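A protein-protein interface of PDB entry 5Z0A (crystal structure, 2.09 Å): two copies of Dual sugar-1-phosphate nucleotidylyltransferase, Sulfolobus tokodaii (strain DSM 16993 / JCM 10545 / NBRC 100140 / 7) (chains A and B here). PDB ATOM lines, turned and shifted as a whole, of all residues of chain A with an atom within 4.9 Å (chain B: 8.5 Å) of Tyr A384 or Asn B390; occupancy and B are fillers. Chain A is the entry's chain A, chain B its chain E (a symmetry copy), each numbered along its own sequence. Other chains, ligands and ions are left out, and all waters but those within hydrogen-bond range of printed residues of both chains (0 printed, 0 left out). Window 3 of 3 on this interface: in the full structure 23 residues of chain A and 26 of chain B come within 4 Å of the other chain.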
ATOM      1  N   GLY A 366     -14.642  28.626  25.757  1.00  0.00           N
ATOM      2  CA  GLY A 366     -13.449  28.867  24.920  1.00  0.00           C
ATOM      3  C   GLY A 366     -13.833  29.796  23.763  1.00  0.00           C
ATOM      4  O   GLY A 366     -15.040  30.094  23.496  1.00  0.00           O
ATOM      5  N   VAL A 369     -17.033  29.355  20.487  1.00  0.00           N
ATOM      6  CA  VAL A 369     -18.108  28.475  20.921  1.00  0.00           C
ATOM      7  C   VAL A 369     -19.472  28.911  20.391  1.00  0.00           C
ATOM      8  O   VAL A 369     -19.785  30.092  20.350  1.00  0.00           O
ATOM      9  CB  VAL A 369     -18.062  28.419  22.445  1.00  0.00           C
ATOM     10  CG1 VAL A 369     -19.344  27.908  23.058  1.00  0.00           C
ATOM     11  CG2 VAL A 369     -16.872  27.543  22.825  1.00  0.00           C
ATOM     12  N   ARG A 382     -16.968  23.867  31.498  1.00  0.00           N
ATOM     13  CA  ARG A 382     -15.987  24.446  30.588  1.00  0.00           C
ATOM     14  C   ARG A 382     -16.315  24.008  29.196  1.00  0.00           C
ATOM     15  O   ARG A 382     -16.610  22.843  28.972  1.00  0.00           O
ATOM     16  CB  ARG A 382     -14.573  24.049  30.966  1.00  0.00           C
ATOM     17  CG  ARG A 382     -14.206  24.693  32.305  1.00  0.00           C
ATOM     18  CD  ARG A 382     -13.545  23.840  33.374  1.00  0.00           C
ATOM     19  NE  ARG A 382     -12.220  23.292  33.049  1.00  0.00           N
ATOM     20  CZ  ARG A 382     -11.018  23.647  33.561  1.00  0.00           C
ATOM     21  NH1 ARG A 382      -9.924  23.006  33.125  1.00  0.00           N
ATOM     22  NH2 ARG A 382     -10.868  24.606  34.495  1.00  0.00           N
ATOM     23  N   ILE A 383     -16.388  24.952  28.267  1.00  0.00           N
ATOM     24  CA  ILE A 383     -16.731  24.573  26.863  1.00  0.00           C
ATOM     25  C   ILE A 383     -15.495  24.784  26.018  1.00  0.00           C
ATOM     26  O   ILE A 383     -15.026  25.908  25.938  1.00  0.00           O
ATOM     27  CB  ILE A 383     -17.914  25.398  26.305  1.00  0.00           C
ATOM     28  CG1 ILE A 383     -19.091  25.436  27.269  1.00  0.00           C
ATOM     29  CG2 ILE A 383     -18.357  24.885  24.937  1.00  0.00           C
ATOM     30  CD1 ILE A 383     -19.704  24.096  27.718  1.00  0.00           C
ATOM     31  N   TYR A 384     -15.027  23.726  25.345  1.00  0.00           N
ATOM     32  CA  TYR A 384     -13.735  23.729  24.605  1.00  0.00           C
ATOM     33  C   TYR A 384     -13.837  24.632  23.356  1.00  0.00           C
ATOM     34  O   TYR A 384     -14.914  24.688  22.747  1.00  0.00           O
ATOM     35  CB  TYR A 384     -13.437  22.283  24.112  1.00  0.00           C
ATOM     36  CG  TYR A 384     -12.058  22.084  23.471  1.00  0.00           C
ATOM     37  CD1 TYR A 384     -10.922  21.905  24.265  1.00  0.00           C
ATOM     38  CD2 TYR A 384     -11.904  22.086  22.056  1.00  0.00           C
ATOM     39  CE1 TYR A 384      -9.652  21.763  23.685  1.00  0.00           C
ATOM     40  CE2 TYR A 384     -10.657  21.935  21.460  1.00  0.00           C
ATOM     41  CZ  TYR A 384      -9.526  21.776  22.278  1.00  0.00           C
ATOM     42  OH  TYR A 384      -8.274  21.610  21.752  1.00  0.00           O
ATOM     43  N   PRO A 385     -12.747  25.372  23.004  1.00  0.00           N
ATOM     44  CA  PRO A 385     -12.774  26.217  21.825  1.00  0.00           C
ATOM     45  C   PRO A 385     -13.389  25.552  20.602  1.00  0.00           C
ATOM     46  O   PRO A 385     -13.115  24.398  20.338  1.00  0.00           O
ATOM     47  CB  PRO A 385     -11.297  26.495  21.581  1.00  0.00           C
ATOM     48  CG  PRO A 385     -10.737  26.639  23.003  1.00  0.00           C
ATOM     49  CD  PRO A 385     -11.433  25.442  23.688  1.00  0.00           C
ATOM     50  N   GLY A 386     -14.257  26.262  19.921  1.00  0.00           N
ATOM     51  CA  GLY A 386     -14.847  25.732  18.683  1.00  0.00           C
ATOM     52  C   GLY A 386     -16.008  24.750  18.882  1.00  0.00           C
ATOM     53  O   GLY A 386     -16.652  24.400  17.931  1.00  0.00           O
ATOM     54  N   ALA A 387     -16.399  24.449  20.124  1.00  0.00           N
ATOM     55  CA  ALA A 387     -17.464  23.474  20.310  1.00  0.00           C
ATOM     56  C   ALA A 387     -18.828  23.989  19.894  1.00  0.00           C
ATOM     57  O   ALA A 387     -19.146  25.191  20.025  1.00  0.00           O
ATOM     58  CB  ALA A 387     -17.494  22.995  21.749  1.00  0.00           C
ATOM     59  N   PHE A 398     -16.757  19.233  31.387  1.00  0.00           N
ATOM     60  CA  PHE A 398     -15.836  19.741  30.337  1.00  0.00           C
ATOM     61  C   PHE A 398     -16.361  19.262  28.964  1.00  0.00           C
ATOM     62  O   PHE A 398     -16.199  18.097  28.604  1.00  0.00           O
ATOM     63  CB  PHE A 398     -14.358  19.369  30.632  1.00  0.00           C
ATOM     64  CG  PHE A 398     -13.298  20.195  29.845  1.00  0.00           C
ATOM     65  CD1 PHE A 398     -13.592  20.915  28.672  1.00  0.00           C
ATOM     66  CD2 PHE A 398     -11.944  20.191  30.273  1.00  0.00           C
ATOM     67  CE1 PHE A 398     -12.598  21.638  27.971  1.00  0.00           C
ATOM     68  CE2 PHE A 398     -10.944  20.913  29.569  1.00  0.00           C
ATOM     69  CZ  PHE A 398     -11.272  21.620  28.407  1.00  0.00           C
ATOM     70  N   PHE A 399     -17.063  20.142  28.261  1.00  0.00           N
ATOM     71  CA  PHE A 399     -17.718  19.801  26.988  1.00  0.00           C
ATOM     72  C   PHE A 399     -16.694  19.966  25.825  1.00  0.00           C
ATOM     73  O   PHE A 399     -16.188  21.072  25.618  1.00  0.00           O
ATOM     74  CB  PHE A 399     -18.951  20.679  26.754  1.00  0.00           C
ATOM     75  CG  PHE A 399     -19.796  20.280  25.565  1.00  0.00           C
ATOM     76  CD1 PHE A 399     -20.819  19.369  25.696  1.00  0.00           C
ATOM     77  CD2 PHE A 399     -19.554  20.810  24.339  1.00  0.00           C
ATOM     78  CE1 PHE A 399     -21.602  19.030  24.617  1.00  0.00           C
ATOM     79  CE2 PHE A 399     -20.317  20.468  23.220  1.00  0.00           C
ATOM     80  CZ  PHE A 399     -21.334  19.567  23.352  1.00  0.00           C
ATOM     81  N   LYS A 400     -16.388  18.886  25.072  1.00  0.00           N
ATOM     82  CA  LYS A 400     -15.339  18.926  24.007  1.00  0.00           C
ATOM     83  C   LYS A 400     -15.811  18.681  22.588  1.00  0.00           C
ATOM     84  O   LYS A 400     -16.978  18.352  22.372  1.00  0.00           O
ATOM     85  CB  LYS A 400     -14.210  17.962  24.329  1.00  0.00           C
ATOM     86  CG  LYS A 400     -13.286  18.453  25.432  1.00  0.00           C
ATOM     87  CD  LYS A 400     -11.951  17.708  25.402  1.00  0.00           C
ATOM     88  CE  LYS A 400     -11.030  18.167  26.518  1.00  0.00           C
ATOM     89  NZ  LYS A 400     -11.509  17.683  27.845  1.00  0.00           N
ATOM     90  N   PHE B 334      -8.172  27.684  30.760  1.00  0.00           N
ATOM     91  CA  PHE B 334      -9.352  27.618  31.646  1.00  0.00           C
ATOM     92  C   PHE B 334      -8.982  27.695  33.153  1.00  0.00           C
ATOM     93  O   PHE B 334      -9.644  28.387  33.927  1.00  0.00           O
ATOM     94  CB  PHE B 334     -10.114  26.313  31.381  1.00  0.00           C
ATOM     95  CG  PHE B 334     -10.903  26.311  30.124  1.00  0.00           C
ATOM     96  CD1 PHE B 334     -11.801  27.339  29.865  1.00  0.00           C
ATOM     97  CD2 PHE B 334     -10.764  25.305  29.200  1.00  0.00           C
ATOM     98  CE1 PHE B 334     -12.555  27.329  28.689  1.00  0.00           C
ATOM     99  CE2 PHE B 334     -11.510  25.301  28.040  1.00  0.00           C
ATOM    100  CZ  PHE B 334     -12.414  26.306  27.797  1.00  0.00           C
ATOM    101  N   ASN B 342       6.039  24.851  23.411  1.00  0.00           N
ATOM    102  CA  ASN B 342       7.132  23.944  22.979  1.00  0.00           C
ATOM    103  C   ASN B 342       8.305  24.736  22.373  1.00  0.00           C
ATOM    104  O   ASN B 342       8.155  25.411  21.372  1.00  0.00           O
ATOM    105  CB  ASN B 342       6.631  22.857  22.015  1.00  0.00           C
ATOM    106  CG  ASN B 342       5.472  22.108  22.596  1.00  0.00           C
ATOM    107  OD1 ASN B 342       5.498  21.704  23.755  1.00  0.00           O
ATOM    108  ND2 ASN B 342       4.386  21.973  21.809  1.00  0.00           N
ATOM    109  N   ARG B 347       8.505  21.223  26.476  1.00  0.00           N
ATOM    110  CA  ARG B 347       7.356  21.928  26.891  1.00  0.00           C
ATOM    111  C   ARG B 347       7.648  22.759  28.124  1.00  0.00           C
ATOM    112  O   ARG B 347       7.863  22.200  29.192  1.00  0.00           O
ATOM    113  CB  ARG B 347       6.219  20.950  27.153  1.00  0.00           C
ATOM    114  CG  ARG B 347       4.871  21.649  27.323  1.00  0.00           C
ATOM    115  CD  ARG B 347       3.713  20.728  26.939  1.00  0.00           C
ATOM    116  NE  ARG B 347       2.438  21.459  26.916  1.00  0.00           N
ATOM    117  CZ  ARG B 347       2.040  22.303  25.952  1.00  0.00           C
ATOM    118  NH1 ARG B 347       2.820  22.621  24.893  1.00  0.00           N
ATOM    119  NH2 ARG B 347       0.852  22.899  26.082  1.00  0.00           N
ATOM    120  N   THR B 370      -9.646  29.011  14.641  1.00  0.00           N
ATOM    121  CA  THR B 370      -9.554  29.086  16.126  1.00  0.00           C
ATOM    122  C   THR B 370      -8.136  28.635  16.457  1.00  0.00           C
ATOM    123  O   THR B 370      -7.739  27.472  16.129  1.00  0.00           O
ATOM    124  CB  THR B 370     -10.569  28.103  16.690  1.00  0.00           C
ATOM    125  OG1 THR B 370     -11.888  28.555  16.389  1.00  0.00           O
ATOM    126  CG2 THR B 370     -10.468  27.914  18.185  1.00  0.00           C
ATOM    127  N   ILE B 371      -7.365  29.482  17.137  1.00  0.00           N
ATOM    128  CA  ILE B 371      -5.984  29.127  17.556  1.00  0.00           C
ATOM    129  C   ILE B 371      -5.833  29.111  19.109  1.00  0.00           C
ATOM    130  O   ILE B 371      -6.138  30.090  19.748  1.00  0.00           O
ATOM    131  CB  ILE B 371      -4.969  30.112  16.943  1.00  0.00           C
ATOM    132  CG1 ILE B 371      -5.103  30.161  15.384  1.00  0.00           C
ATOM    133  CG2 ILE B 371      -3.566  29.742  17.379  1.00  0.00           C
ATOM    134  CD1 ILE B 371      -4.340  31.286  14.730  1.00  0.00           C
ATOM    135  N   LEU B 372      -5.283  28.015  19.662  1.00  0.00           N
ATOM    136  CA  LEU B 372      -5.208  27.830  21.112  1.00  0.00           C
ATOM    137  C   LEU B 372      -3.985  28.515  21.725  1.00  0.00           C
ATOM    138  O   LEU B 372      -3.023  28.816  21.034  1.00  0.00           O
ATOM    139  CB  LEU B 372      -5.259  26.319  21.446  1.00  0.00           C
ATOM    140  CG  LEU B 372      -6.678  25.825  21.710  1.00  0.00           C
ATOM    141  CD1 LEU B 372      -7.639  26.064  20.564  1.00  0.00           C
ATOM    142  CD2 LEU B 372      -6.698  24.384  22.126  1.00  0.00           C
ATOM    143  N   PRO B 373      -4.000  28.732  23.046  1.00  0.00           N
ATOM    144  CA  PRO B 373      -2.884  29.455  23.669  1.00  0.00           C
ATOM    145  C   PRO B 373      -1.521  28.734  23.587  1.00  0.00           C
ATOM    146  O   PRO B 373      -1.471  27.552  23.789  1.00  0.00           O
ATOM    147  CB  PRO B 373      -3.308  29.515  25.118  1.00  0.00           C
ATOM    148  CG  PRO B 373      -4.794  29.309  25.113  1.00  0.00           C
ATOM    149  CD  PRO B 373      -4.986  28.289  24.052  1.00  0.00           C
ATOM    150  N   GLY B 374      -0.482  29.485  23.280  1.00  0.00           N
ATOM    151  CA  GLY B 374       0.868  29.019  23.246  1.00  0.00           C
ATOM    152  C   GLY B 374       1.289  28.272  21.971  1.00  0.00           C
ATOM    153  O   GLY B 374       2.403  27.803  21.887  1.00  0.00           O
ATOM    154  N   VAL B 375       0.389  28.184  20.998  1.00  0.00           N
ATOM    155  CA  VAL B 375       0.617  27.447  19.797  1.00  0.00           C
ATOM    156  C   VAL B 375       1.611  28.179  18.907  1.00  0.00           C
ATOM    157  O   VAL B 375       1.552  29.403  18.738  1.00  0.00           O
ATOM    158  CB  VAL B 375      -0.751  27.255  19.087  1.00  0.00           C
ATOM    159  CG1 VAL B 375      -0.658  27.002  17.609  1.00  0.00           C
ATOM    160  CG2 VAL B 375      -1.505  26.144  19.799  1.00  0.00           C
ATOM    161  N   LYS B 376       2.471  27.423  18.272  1.00  0.00           N
ATOM    162  CA  LYS B 376       3.383  27.956  17.223  1.00  0.00           C
ATOM    163  C   LYS B 376       2.927  27.486  15.837  1.00  0.00           C
ATOM    164  O   LYS B 376       2.642  26.293  15.651  1.00  0.00           O
ATOM    165  CB  LYS B 376       4.779  27.455  17.489  1.00  0.00           C
ATOM    166  CG  LYS B 376       5.385  28.070  18.738  1.00  0.00           C
ATOM    167  CD  LYS B 376       6.581  27.321  19.298  1.00  0.00           C
ATOM    168  CE  LYS B 376       7.523  26.813  18.247  1.00  0.00           C
ATOM    169  NZ  LYS B 376       8.724  26.165  18.874  1.00  0.00           N
ATOM    170  N   ILE B 377       2.865  28.429  14.888  1.00  0.00           N
ATOM    171  CA  ILE B 377       2.494  28.092  13.516  1.00  0.00           C
ATOM    172  C   ILE B 377       3.688  28.448  12.642  1.00  0.00           C
ATOM    173  O   ILE B 377       4.064  29.625  12.490  1.00  0.00           O
ATOM    174  CB  ILE B 377       1.185  28.758  13.047  1.00  0.00           C
ATOM    175  CG1 ILE B 377       0.057  28.315  13.929  1.00  0.00           C
ATOM    176  CG2 ILE B 377       0.884  28.441  11.568  1.00  0.00           C
ATOM    177  CD1 ILE B 377      -1.307  28.860  13.575  1.00  0.00           C
ATOM    178  N   ILE B 383      -3.804  27.433   7.297  1.00  0.00           N
ATOM    179  CA  ILE B 383      -4.821  26.849   8.149  1.00  0.00           C
ATOM    180  C   ILE B 383      -6.178  26.892   7.483  1.00  0.00           C
ATOM    181  O   ILE B 383      -6.707  27.949   7.140  1.00  0.00           O
ATOM    182  CB  ILE B 383      -4.887  27.572   9.486  1.00  0.00           C
ATOM    183  CG1 ILE B 383      -3.501  27.813  10.053  1.00  0.00           C
ATOM    184  CG2 ILE B 383      -5.773  26.832  10.469  1.00  0.00           C
ATOM    185  CD1 ILE B 383      -2.600  26.583  10.283  1.00  0.00           C
ATOM    186  N   ALA B 387     -10.787  25.522  11.029  1.00  0.00           N
ATOM    187  CA  ALA B 387      -9.957  24.587  11.803  1.00  0.00           C
ATOM    188  C   ALA B 387      -9.710  25.078  13.230  1.00  0.00           C
ATOM    189  O   ALA B 387      -9.694  26.285  13.506  1.00  0.00           O
ATOM    190  CB  ALA B 387      -8.625  24.366  11.108  1.00  0.00           C
ATOM    191  N   VAL B 388      -9.573  24.114  14.133  1.00  0.00           N
ATOM    192  CA  VAL B 388      -9.187  24.369  15.492  1.00  0.00           C
ATOM    193  C   VAL B 388      -7.729  23.987  15.637  1.00  0.00           C
ATOM    194  O   VAL B 388      -7.343  22.792  15.630  1.00  0.00           O
ATOM    195  CB  VAL B 388     -10.082  23.595  16.480  1.00  0.00           C
ATOM    196  CG1 VAL B 388      -9.659  23.883  17.888  1.00  0.00           C
ATOM    197  CG2 VAL B 388     -11.563  23.963  16.283  1.00  0.00           C
ATOM    198  N   VAL B 389      -6.877  24.985  15.752  1.00  0.00           N
ATOM    199  CA  VAL B 389      -5.402  24.727  15.828  1.00  0.00           C
ATOM    200  C   VAL B 389      -5.020  24.478  17.281  1.00  0.00           C
ATOM    201  O   VAL B 389      -4.805  25.411  18.061  1.00  0.00           O
ATOM    202  CB  VAL B 389      -4.571  25.866  15.239  1.00  0.00           C
ATOM    203  CG1 VAL B 389      -3.078  25.470  15.175  1.00  0.00           C
ATOM    204  CG2 VAL B 389      -5.061  26.232  13.827  1.00  0.00           C
ATOM    205  N   ASN B 390      -4.988  23.203  17.645  1.00  0.00           N
ATOM    206  CA  ASN B 390      -4.727  22.780  19.038  1.00  0.00           C
ATOM    207  C   ASN B 390      -3.354  22.114  19.213  1.00  0.00           C
ATOM    208  O   ASN B 390      -3.144  21.457  20.200  1.00  0.00           O
ATOM    209  CB  ASN B 390      -5.822  21.844  19.514  1.00  0.00           C
ATOM    210  CG  ASN B 390      -5.943  20.565  18.654  1.00  0.00           C
ATOM    211  OD1 ASN B 390      -5.277  20.375  17.617  1.00  0.00           O
ATOM    212  ND2 ASN B 390      -6.857  19.723  19.051  1.00  0.00           N
ATOM    213  N   ARG B 391      -2.426  22.315  18.262  1.00  0.00           N
ATOM    214  CA  ARG B 391      -1.016  21.891  18.424  1.00  0.00           C
ATOM    215  C   ARG B 391      -0.160  22.796  17.539  1.00  0.00           C
ATOM    216  O   ARG B 391      -0.688  23.481  16.654  1.00  0.00           O
ATOM    217  CB  ARG B 391      -0.838  20.400  18.020  1.00  0.00           C
ATOM    218  CG  ARG B 391      -1.538  20.059  16.700  1.00  0.00           C
ATOM    219  CD  ARG B 391      -1.102  18.741  16.004  1.00  0.00           C
ATOM    220  NE  ARG B 391      -0.281  19.220  14.964  1.00  0.00           N
ATOM    221  CZ  ARG B 391      -0.448  19.187  13.654  1.00  0.00           C
ATOM    222  NH1 ARG B 391      -1.343  18.470  13.046  1.00  0.00           N
ATOM    223  NH2 ARG B 391       0.476  19.804  12.958  1.00  0.00           N
ATOM    224  N   ASP B 392       1.154  22.679  17.673  1.00  0.00           N
ATOM    225  CA  ASP B 392       2.100  23.342  16.777  1.00  0.00           C
ATOM    226  C   ASP B 392       1.953  22.843  15.341  1.00  0.00           C
ATOM    227  O   ASP B 392       1.619  21.685  15.094  1.00  0.00           O
ATOM    228  CB  ASP B 392       3.540  23.164  17.251  1.00  0.00           C
ATOM    229  CG  ASP B 392       3.780  23.828  18.623  1.00  0.00           C
ATOM    230  OD1 ASP B 392       2.930  24.680  19.084  1.00  0.00           O
ATOM    231  OD2 ASP B 392       4.721  23.379  19.287  1.00  0.00           O
ATOM    232  N   VAL B 393       2.134  23.774  14.415  1.00  0.00           N
ATOM    233  CA  VAL B 393       1.926  23.483  12.979  1.00  0.00           C
ATOM    234  C   VAL B 393       3.267  23.684  12.329  1.00  0.00           C
ATOM    235  O   VAL B 393       3.936  24.683  12.573  1.00  0.00           O
ATOM    236  CB  VAL B 393       0.849  24.420  12.363  1.00  0.00           C
ATOM    237  CG1 VAL B 393       0.723  24.205  10.862  1.00  0.00           C
ATOM    238  CG2 VAL B 393      -0.510  24.179  13.053  1.00  0.00           C
ATOM    239  N   PHE B 399      -2.770  22.715   7.415  1.00  0.00           N
ATOM    240  CA  PHE B 399      -3.484  22.168   8.546  1.00  0.00           C
ATOM    241  C   PHE B 399      -4.946  22.081   8.181  1.00  0.00           C
ATOM    242  O   PHE B 399      -5.605  23.140   8.015  1.00  0.00           O
ATOM    243  CB  PHE B 399      -3.249  23.039   9.794  1.00  0.00           C
ATOM    244  CG  PHE B 399      -3.789  22.468  11.056  1.00  0.00           C
ATOM    245  CD1 PHE B 399      -2.997  21.642  11.873  1.00  0.00           C
ATOM    246  CD2 PHE B 399      -5.095  22.759  11.483  1.00  0.00           C
ATOM    247  CE1 PHE B 399      -3.507  21.129  13.054  1.00  0.00           C
ATOM    248  CE2 PHE B 399      -5.615  22.226  12.661  1.00  0.00           C
ATOM    249  CZ  PHE B 399      -4.824  21.411  13.453  1.00  0.00           C
ATOM    250  N   LYS B 400      -5.507  20.853   8.153  1.00  0.00           N
ATOM    251  CA  LYS B 400      -6.957  20.648   7.838  1.00  0.00           C
ATOM    252  C   LYS B 400      -7.850  20.036   8.895  1.00  0.00           C
ATOM    253  O   LYS B 400      -7.452  19.838  10.056  1.00  0.00           O
ATOM    254  CB  LYS B 400      -7.083  19.784   6.626  1.00  0.00           C
ATOM    255  CG  LYS B 400      -6.683  20.492   5.351  1.00  0.00           C
ATOM    256  CD  LYS B 400      -7.200  19.729   4.143  1.00  0.00           C
ATOM    257  CE  LYS B 400      -6.809  20.415   2.846  1.00  0.00           C
ATOM    258  NZ  LYS B 400      -5.347  20.272   2.577  1.00  0.00           N
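N of Phe A399 lies within hydrogen-bond range of O of Arg A382, at 2.8 Å.
N of Leu B372 sits at hydrogen-bond distance from O of Val B389, 3.1 Å away.
O of Ala B387 lies within hydrogen-bond range of N of Thr B370 (3.0 Å).
The backbone carbonyl oxygen (O) of Phe A399 lies within hydrogen-bond range of the backbone NH (N) of Tyr A384, at 2.9 Å.
N of Gly A366 sits at hydrogen-bond distance from O of Ile A383, 2.8 Å away.
N of Val B389 lies within hydrogen-bond range of O of Thr B370 (2.7 Å).
Among the printed residues, pairs that only touch across the chains: Tyr A384 with Leu B372, Ile A383 with Phe B334, Tyr A384 with Asn B390, Arg A382 with Phe B334, Phe A398 with Phe B334, Pro A385 with Thr B370, Gly A366 with Phe B334 and Pro A385 with Leu B372.
Of the printed residues of chain B, Gly A366 touches Phe B334 (3.8 Å).
Of chain B, only Leu B372 (3.2 Å) and Asn B390 (3.3 Å) come within 4 Å of Tyr A384.
Of chain B, only Thr B370 and Leu B372 come within 4 Å of Pro A385.
Of the printed residues of chain B, Phe A398 touches Phe B334.
Of the printed residues of chain A, Phe B334 touches Gly A366 (3.8 Å), Arg A382 (3.6 Å), Ile A383 (3.2 Å) and Phe A398 (3.7 Å).
Of the printed residues of chain A, Leu B372 touches Tyr A384 and Pro A385.
Val B388 touches none of the printed residues of chain A.
Asn B390 touches just one residue of chain A: Tyr A384.
The nearest residue of chain B that does not touch Tyr A384 is Val B388 (4.2 Å).
The nearest printed residue of chain B that does not touch Gly A366 is Thr B370 (6.8 Å).
Printed residues of chain A that touch a printed residue of chain B: Gly A366, Arg A382, Ile A383, Tyr A384, Pro A385 and Phe A398.
Hydrophobic or aromatic side chains of chain A that line the printed part of chain B: Tyr A384, Pro A385 and Phe A398.
Along chain A the printed residues that touch a printed residue of chain B span positions 366 to 398.
Hydrophobic or aromatic side chains of chain B that line the printed part of chain A: Phe B334 and Leu B372.
Along chain B the printed residues that touch a printed residue of chain A span positions 334 to 390.
4 positions are printed for both chains.
Of the 8 pairs that touch across the chains among the printed residues, none has its exchanged pair printed and touching as well.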
